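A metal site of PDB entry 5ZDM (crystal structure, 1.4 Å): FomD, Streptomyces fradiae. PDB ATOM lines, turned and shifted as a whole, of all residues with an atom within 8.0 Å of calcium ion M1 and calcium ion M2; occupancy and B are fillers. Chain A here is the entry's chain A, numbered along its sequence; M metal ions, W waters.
The side-chain amide nitrogen (ND2) of Asn 113 lies within hydrogen-bond range of the side-chain carboxylate (OE1) of Glu 115 (2.8 Å).
N of Glu 131 lies within hydrogen-bond range of OD2 of Asp 129 (2.9 Å).
NZ of Lys 150 lies within salt-bridge range of OE2 of Glu 131 (3.0 Å).
The guanidinium group (NH1) of Arg 154 lies within salt-bridge range of the side-chain carboxylate (OE2) of Glu 131.
The backbone carbonyl oxygen (O) of Asp 133 lies within hydrogen-bond range of the backbone NH (N) of Lys 146 (2.8 Å).
The side-chain carboxylate (OD1) of Asp 133 sits close to the side-chain hydroxyl (OH) of Tyr 111, at 3.2 Å.
The backbone NH (N) of Asp 129 is in hydrogen-bond range of the side-chain carboxylate (OD2) of Asp 26, 2.9 Å away.
The side-chain hydroxyl (OH) of Tyr 111 lies within hydrogen-bond range of the side-chain amino group (NZ) of Lys 146.
Three residues have an atom within 4 Å of calcium ion M1: Asn 113, Asp 129 and Asp 133.
The nearest printed residue that does not touch calcium ion M1 is Glu 131 (4.2 Å).
Merely in contact with calcium ion M2: Lys 146 (3.9 Å).
The side-chain amide oxygen (OD1) of Asn 113 binds calcium ion M1.
OD1 of Asp 129 is bound to calcium ion M1, at 2.4 Å.
The side-chain carboxylate (OD1) of Asp 133 binds calcium ion M1 (2.4 Å).
Calcium ion M1 is bound by water W2, 2.4 Å away.
Calcium ion M1 is bound by water W1 (2.4 Å).
Calcium ion M2 is bound by the backbone carbonyl oxygen (O) of Glu 131, the side-chain carboxylate (OE1) of Glu 131, the side-chain carboxylate (OD2) of Asp 147, the side-chain carboxylate (OD2) of Asp 133, water W1 and the side-chain carboxylate (OD1) of Asp 133.
Calcium ion M2 has six donor atoms within binding distance.
Water W2 lies within hydrogen-bond range of O of Ile 132, O of Val 114 and N of Glu 131.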
ATOM      1  N   ASP A  26     -32.091  28.243  -0.799  1.00  0.00           N
ATOM      2  CA  ASP A  26     -32.439  27.168  -1.695  1.00  0.00           C
ATOM      3  C   ASP A  26     -33.466  26.281  -0.982  1.00  0.00           C
ATOM      4  O   ASP A  26     -33.160  25.826   0.150  1.00  0.00           O
ATOM      5  CB  ASP A  26     -31.264  26.229  -2.134  1.00  0.00           C
ATOM      6  CG  ASP A  26     -30.308  26.857  -3.048  1.00  0.00           C
ATOM      7  OD1 ASP A  26     -29.636  27.813  -2.666  1.00  0.00           O
ATOM      8  OD2 ASP A  26     -30.209  26.395  -4.181  1.00  0.00           O
ATOM      9  N   TRP A  97     -22.976  34.844 -10.844  1.00  0.00           N
ATOM     10  CA  TRP A  97     -22.126  35.117  -9.678  1.00  0.00           C
ATOM     11  C   TRP A  97     -20.812  35.708 -10.162  1.00  0.00           C
ATOM     12  O   TRP A  97     -20.185  35.209 -11.119  1.00  0.00           O
ATOM     13  CB  TRP A  97     -21.851  33.836  -8.937  1.00  0.00           C
ATOM     14  CG  TRP A  97     -23.045  33.164  -8.384  1.00  0.00           C
ATOM     15  CD1 TRP A  97     -24.366  33.492  -8.539  1.00  0.00           C
ATOM     16  CD2 TRP A  97     -23.039  31.959  -7.590  1.00  0.00           C
ATOM     17  NE1 TRP A  97     -25.188  32.583  -7.892  1.00  0.00           N
ATOM     18  CE2 TRP A  97     -24.384  31.659  -7.248  1.00  0.00           C
ATOM     19  CE3 TRP A  97     -22.026  31.112  -7.157  1.00  0.00           C
ATOM     20  CZ2 TRP A  97     -24.730  30.526  -6.552  1.00  0.00           C
ATOM     21  CZ3 TRP A  97     -22.351  30.014  -6.427  1.00  0.00           C
ATOM     22  CH2 TRP A  97     -23.713  29.755  -6.084  1.00  0.00           C
ATOM     23  N   TYR A 111     -19.937  33.225 -13.144  1.00  0.00           N
ATOM     24  CA  TYR A 111     -20.434  31.833 -12.920  1.00  0.00           C
ATOM     25  C   TYR A 111     -21.949  31.844 -13.008  1.00  0.00           C
ATOM     26  O   TYR A 111     -22.610  32.405 -12.177  1.00  0.00           O
ATOM     27  CB  TYR A 111     -19.879  31.324 -11.656  1.00  0.00           C
ATOM     28  CG  TYR A 111     -20.132  29.857 -11.375  1.00  0.00           C
ATOM     29  CD1 TYR A 111     -19.264  28.945 -11.821  1.00  0.00           C
ATOM     30  CD2 TYR A 111     -21.262  29.440 -10.680  1.00  0.00           C
ATOM     31  CE1 TYR A 111     -19.502  27.594 -11.578  1.00  0.00           C
ATOM     32  CE2 TYR A 111     -21.469  28.093 -10.385  1.00  0.00           C
ATOM     33  CZ  TYR A 111     -20.595  27.177 -10.873  1.00  0.00           C
ATOM     34  OH  TYR A 111     -20.707  25.803 -10.618  1.00  0.00           O
ATOM     35  N   VAL A 112     -22.455  31.306 -14.096  1.00  0.00           N
ATOM     36  CA  VAL A 112     -23.902  31.281 -14.355  1.00  0.00           C
ATOM     37  C   VAL A 112     -24.488  30.045 -13.605  1.00  0.00           C
ATOM     38  O   VAL A 112     -24.186  28.918 -13.973  1.00  0.00           O
ATOM     39  CB  VAL A 112     -24.256  31.204 -15.812  1.00  0.00           C
ATOM     40  CG1 VAL A 112     -25.760  31.228 -15.986  1.00  0.00           C
ATOM     41  CG2 VAL A 112     -23.587  32.378 -16.553  1.00  0.00           C
ATOM     42  N   ASN A 113     -25.254  30.302 -12.559  1.00  0.00           N
ATOM     43  CA  ASN A 113     -25.858  29.271 -11.781  1.00  0.00           C
ATOM     44  C   ASN A 113     -27.288  29.112 -12.196  1.00  0.00           C
ATOM     45  O   ASN A 113     -28.157  29.894 -11.842  1.00  0.00           O
ATOM     46  CB  ASN A 113     -25.729  29.705 -10.279  1.00  0.00           C
ATOM     47  CG  ASN A 113     -25.783  28.428  -9.397  1.00  0.00           C
ATOM     48  OD1 ASN A 113     -24.906  27.578  -9.565  1.00  0.00           O
ATOM     49  ND2 ASN A 113     -26.932  28.257  -8.620  1.00  0.00           N
ATOM     50  N   VAL A 114     -27.571  28.059 -12.978  1.00  0.00           N
ATOM     51  CA  VAL A 114     -28.930  27.784 -13.427  1.00  0.00           C
ATOM     52  C   VAL A 114     -29.691  27.262 -12.220  1.00  0.00           C
ATOM     53  O   VAL A 114     -29.153  26.437 -11.448  1.00  0.00           O
ATOM     54  CB  VAL A 114     -28.870  26.750 -14.581  1.00  0.00           C
ATOM     55  CG1 VAL A 114     -30.250  26.466 -15.117  1.00  0.00           C
ATOM     56  CG2 VAL A 114     -27.986  27.316 -15.708  1.00  0.00           C
ATOM     57  N   GLU A 115     -30.831  27.808 -11.992  1.00  0.00           N
ATOM     58  CA  GLU A 115     -31.616  27.635 -10.737  1.00  0.00           C
ATOM     59  C   GLU A 115     -32.992  28.182 -10.937  1.00  0.00           C
ATOM     60  O   GLU A 115     -33.274  28.950 -11.933  1.00  0.00           O
ATOM     61  CB  GLU A 115     -30.896  28.325  -9.579  1.00  0.00           C
ATOM     62  CG  GLU A 115     -30.772  29.868  -9.742  1.00  0.00           C
ATOM     63  CD  GLU A 115     -29.919  30.464  -8.719  1.00  0.00           C
ATOM     64  OE1 GLU A 115     -29.166  29.813  -7.981  1.00  0.00           O
ATOM     65  OE2 GLU A 115     -29.865  31.761  -8.720  1.00  0.00           O
ATOM     66  N   LEU A 128     -33.671  27.413  -6.120  1.00  0.00           N
ATOM     67  CA  LEU A 128     -33.180  26.044  -5.997  1.00  0.00           C
ATOM     68  C   LEU A 128     -32.194  25.738  -7.108  1.00  0.00           C
ATOM     69  O   LEU A 128     -32.551  25.929  -8.251  1.00  0.00           O
ATOM     70  CB  LEU A 128     -34.304  24.954  -5.943  1.00  0.00           C
ATOM     71  CG  LEU A 128     -33.816  23.567  -5.845  1.00  0.00           C
ATOM     72  CD1 LEU A 128     -33.025  23.321  -4.554  1.00  0.00           C
ATOM     73  CD2 LEU A 128     -35.003  22.593  -5.959  1.00  0.00           C
ATOM     74  N   ASP A 129     -31.010  25.307  -6.775  1.00  0.00           N
ATOM     75  CA  ASP A 129     -29.965  25.001  -7.779  1.00  0.00           C
ATOM     76  C   ASP A 129     -30.482  23.984  -8.769  1.00  0.00           C
ATOM     77  O   ASP A 129     -31.111  22.959  -8.359  1.00  0.00           O
ATOM     78  CB  ASP A 129     -28.753  24.479  -7.095  1.00  0.00           C
ATOM     79  CG  ASP A 129     -27.605  24.253  -8.002  1.00  0.00           C
ATOM     80  OD1 ASP A 129     -26.874  25.273  -8.302  1.00  0.00           O
ATOM     81  OD2 ASP A 129     -27.401  23.109  -8.510  1.00  0.00           O
ATOM     82  N   HIS A 130     -30.232  24.162 -10.062  1.00  0.00           N
ATOM     83  CA  HIS A 130     -30.652  23.275 -11.157  1.00  0.00           C
ATOM     84  C   HIS A 130     -29.492  22.592 -11.868  1.00  0.00           C
ATOM     85  O   HIS A 130     -29.636  22.144 -13.007  1.00  0.00           O
ATOM     86  CB  HIS A 130     -31.559  23.994 -12.117  1.00  0.00           C
ATOM     87  CG  HIS A 130     -32.922  24.311 -11.577  1.00  0.00           C
ATOM     88  ND1 HIS A 130     -33.816  25.172 -12.212  1.00  0.00           N
ATOM     89  CD2 HIS A 130     -33.538  23.857 -10.476  1.00  0.00           C
ATOM     90  CE1 HIS A 130     -34.936  25.140 -11.524  1.00  0.00           C
ATOM     91  NE2 HIS A 130     -34.776  24.394 -10.466  1.00  0.00           N
ATOM     92  N   GLU A 131     -28.377  22.438 -11.167  1.00  0.00           N
ATOM     93  CA  GLU A 131     -27.179  21.678 -11.508  1.00  0.00           C
ATOM     94  C   GLU A 131     -26.376  22.248 -12.685  1.00  0.00           C
ATOM     95  O   GLU A 131     -25.181  22.413 -12.542  1.00  0.00           O
ATOM     96  CB  GLU A 131     -27.492  20.167 -11.722  1.00  0.00           C
ATOM     97  CG  GLU A 131     -26.226  19.379 -11.924  1.00  0.00           C
ATOM     98  CD  GLU A 131     -25.351  19.425 -10.741  1.00  0.00           C
ATOM     99  OE1 GLU A 131     -24.309  20.117 -10.741  1.00  0.00           O
ATOM    100  OE2 GLU A 131     -25.732  18.725  -9.743  1.00  0.00           O
ATOM    101  N   ILE A 132     -26.939  22.471 -13.840  1.00  0.00           N
ATOM    102  CA  ILE A 132     -26.162  22.988 -14.970  1.00  0.00           C
ATOM    103  C   ILE A 132     -25.560  24.350 -14.554  1.00  0.00           C
ATOM    104  O   ILE A 132     -26.209  25.163 -13.940  1.00  0.00           O
ATOM    105  CB  ILE A 132     -27.023  23.162 -16.256  1.00  0.00           C
ATOM    106  CG1 ILE A 132     -27.675  21.817 -16.643  1.00  0.00           C
ATOM    107  CG2 ILE A 132     -26.148  23.737 -17.401  1.00  0.00           C
ATOM    108  CD1 ILE A 132     -28.403  21.893 -17.935  1.00  0.00           C
ATOM    109  N   ASP A 133     -24.312  24.565 -14.895  1.00  0.00           N
ATOM    110  CA  ASP A 133     -23.649  25.883 -14.685  1.00  0.00           C
ATOM    111  C   ASP A 133     -22.956  26.218 -15.967  1.00  0.00           C
ATOM    112  O   ASP A 133     -22.684  25.406 -16.828  1.00  0.00           O
ATOM    113  CB  ASP A 133     -22.654  25.831 -13.561  1.00  0.00           C
ATOM    114  CG  ASP A 133     -22.895  24.786 -12.525  1.00  0.00           C
ATOM    115  OD1 ASP A 133     -23.686  24.998 -11.614  1.00  0.00           O
ATOM    116  OD2 ASP A 133     -22.310  23.695 -12.647  1.00  0.00           O
ATOM    117  N   LEU A 134     -22.712  27.528 -16.189  1.00  0.00           N
ATOM    118  CA  LEU A 134     -21.872  28.014 -17.306  1.00  0.00           C
ATOM    119  C   LEU A 134     -20.814  28.906 -16.723  1.00  0.00           C
ATOM    120  O   LEU A 134     -21.058  29.570 -15.730  1.00  0.00           O
ATOM    121  CB  LEU A 134     -22.641  28.688 -18.380  1.00  0.00           C
ATOM    122  CG  LEU A 134     -23.925  28.154 -18.957  1.00  0.00           C
ATOM    123  CD1 LEU A 134     -24.433  29.279 -19.909  1.00  0.00           C
ATOM    124  CD2 LEU A 134     -23.629  26.930 -19.606  1.00  0.00           C
ATOM    125  N   LYS A 146     -20.958  23.449 -17.944  1.00  0.00           N
ATOM    126  CA  LYS A 146     -20.495  22.658 -16.799  1.00  0.00           C
ATOM    127  C   LYS A 146     -21.600  21.768 -16.229  1.00  0.00           C
ATOM    128  O   LYS A 146     -22.742  22.211 -16.117  1.00  0.00           O
ATOM    129  CB  LYS A 146     -20.002  23.657 -15.790  1.00  0.00           C
ATOM    130  CG  LYS A 146     -19.411  23.054 -14.530  1.00  0.00           C
ATOM    131  CD  LYS A 146     -18.811  24.089 -13.596  1.00  0.00           C
ATOM    132  CE  LYS A 146     -18.439  23.628 -12.258  1.00  0.00           C
ATOM    133  NZ  LYS A 146     -19.597  23.157 -11.449  1.00  0.00           N
ATOM    134  N   ASP A 147     -21.290  20.546 -15.932  1.00  0.00           N
ATOM    135  CA  ASP A 147     -22.150  19.636 -15.227  1.00  0.00           C
ATOM    136  C   ASP A 147     -23.370  19.210 -15.985  1.00  0.00           C
ATOM    137  O   ASP A 147     -24.376  18.829 -15.378  1.00  0.00           O
ATOM    138  CB  ASP A 147     -22.555  20.228 -13.881  1.00  0.00           C
ATOM    139  CG  ASP A 147     -21.417  20.229 -12.836  1.00  0.00           C
ATOM    140  OD1 ASP A 147     -20.318  19.589 -13.057  1.00  0.00           O
ATOM    141  OD2 ASP A 147     -21.509  20.910 -11.813  1.00  0.00           O
ATOM    142  N   VAL A 148     -23.312  19.245 -17.328  1.00  0.00           N
ATOM    143  CA  VAL A 148     -24.464  18.783 -18.117  1.00  0.00           C
ATOM    144  C   VAL A 148     -24.741  17.280 -17.907  1.00  0.00           C
ATOM    145  O   VAL A 148     -25.856  16.909 -17.651  1.00  0.00           O
ATOM    146  CB  VAL A 148     -24.353  19.091 -19.593  1.00  0.00           C
ATOM    147  CG1 VAL A 148     -25.501  18.499 -20.398  1.00  0.00           C
ATOM    148  CG2 VAL A 148     -24.406  20.625 -19.752  1.00  0.00           C
ATOM    149  N   LYS A 150     -23.773  15.416 -15.433  1.00  0.00           N
ATOM    150  CA  LYS A 150     -24.158  15.247 -14.029  1.00  0.00           C
ATOM    151  C   LYS A 150     -25.649  15.552 -13.863  1.00  0.00           C
ATOM    152  O   LYS A 150     -26.365  14.781 -13.250  1.00  0.00           O
ATOM    153  CB  LYS A 150     -23.309  16.143 -13.158  1.00  0.00           C
ATOM    154  CG  LYS A 150     -23.588  16.014 -11.710  1.00  0.00           C
ATOM    155  CD  LYS A 150     -22.752  17.085 -11.009  1.00  0.00           C
ATOM    156  CE  LYS A 150     -23.099  17.005  -9.558  1.00  0.00           C
ATOM    157  NZ  LYS A 150     -22.890  18.282  -8.936  1.00  0.00           N
ATOM    158  N   PHE A 151     -26.091  16.654 -14.454  1.00  0.00           N
ATOM    159  CA  PHE A 151     -27.507  17.004 -14.478  1.00  0.00           C
ATOM    160  C   PHE A 151     -28.360  15.852 -15.101  1.00  0.00           C
ATOM    161  O   PHE A 151     -29.377  15.480 -14.550  1.00  0.00           O
ATOM    162  CB  PHE A 151     -27.710  18.325 -15.214  1.00  0.00           C
ATOM    163  CG  PHE A 151     -29.121  18.569 -15.605  1.00  0.00           C
ATOM    164  CD1 PHE A 151     -30.054  18.889 -14.669  1.00  0.00           C
ATOM    165  CD2 PHE A 151     -29.495  18.367 -16.918  1.00  0.00           C
ATOM    166  CE1 PHE A 151     -31.410  19.065 -15.028  1.00  0.00           C
ATOM    167  CE2 PHE A 151     -30.831  18.579 -17.281  1.00  0.00           C
ATOM    168  CZ  PHE A 151     -31.733  18.921 -16.343  1.00  0.00           C
ATOM    169  N   ARG A 154     -28.744  12.952 -12.787  1.00  0.00           N
ATOM    170  CA  ARG A 154     -29.728  13.246 -11.821  1.00  0.00           C
ATOM    171  C   ARG A 154     -31.148  13.324 -12.322  1.00  0.00           C
ATOM    172  O   ARG A 154     -32.077  12.857 -11.573  1.00  0.00           O
ATOM    173  CB  ARG A 154     -29.309  14.581 -11.112  1.00  0.00           C
ATOM    174  CG  ARG A 154     -28.026  14.461 -10.342  1.00  0.00           C
ATOM    175  CD  ARG A 154     -27.582  15.778  -9.589  1.00  0.00           C
ATOM    176  NE  ARG A 154     -28.628  16.116  -8.663  1.00  0.00           N
ATOM    177  CZ  ARG A 154     -28.963  17.332  -8.266  1.00  0.00           C
ATOM    178  NH1 ARG A 154     -28.255  18.388  -8.691  1.00  0.00           N
ATOM    179  NH2 ARG A 154     -29.981  17.478  -7.454  1.00  0.00           N
HETATM  180 CA    CA M   1     -24.867  25.369  -9.578  1.00  0.00          CA
HETATM  181 CA    CA M   2     -23.377  22.202 -11.139  1.00  0.00          CA
HETATM  182  O   HOH W   1     -24.817  22.967  -9.199  1.00  0.00           O
HETATM  183  O   HOH W   2     -26.586  25.330 -11.246  1.00  0.00           O
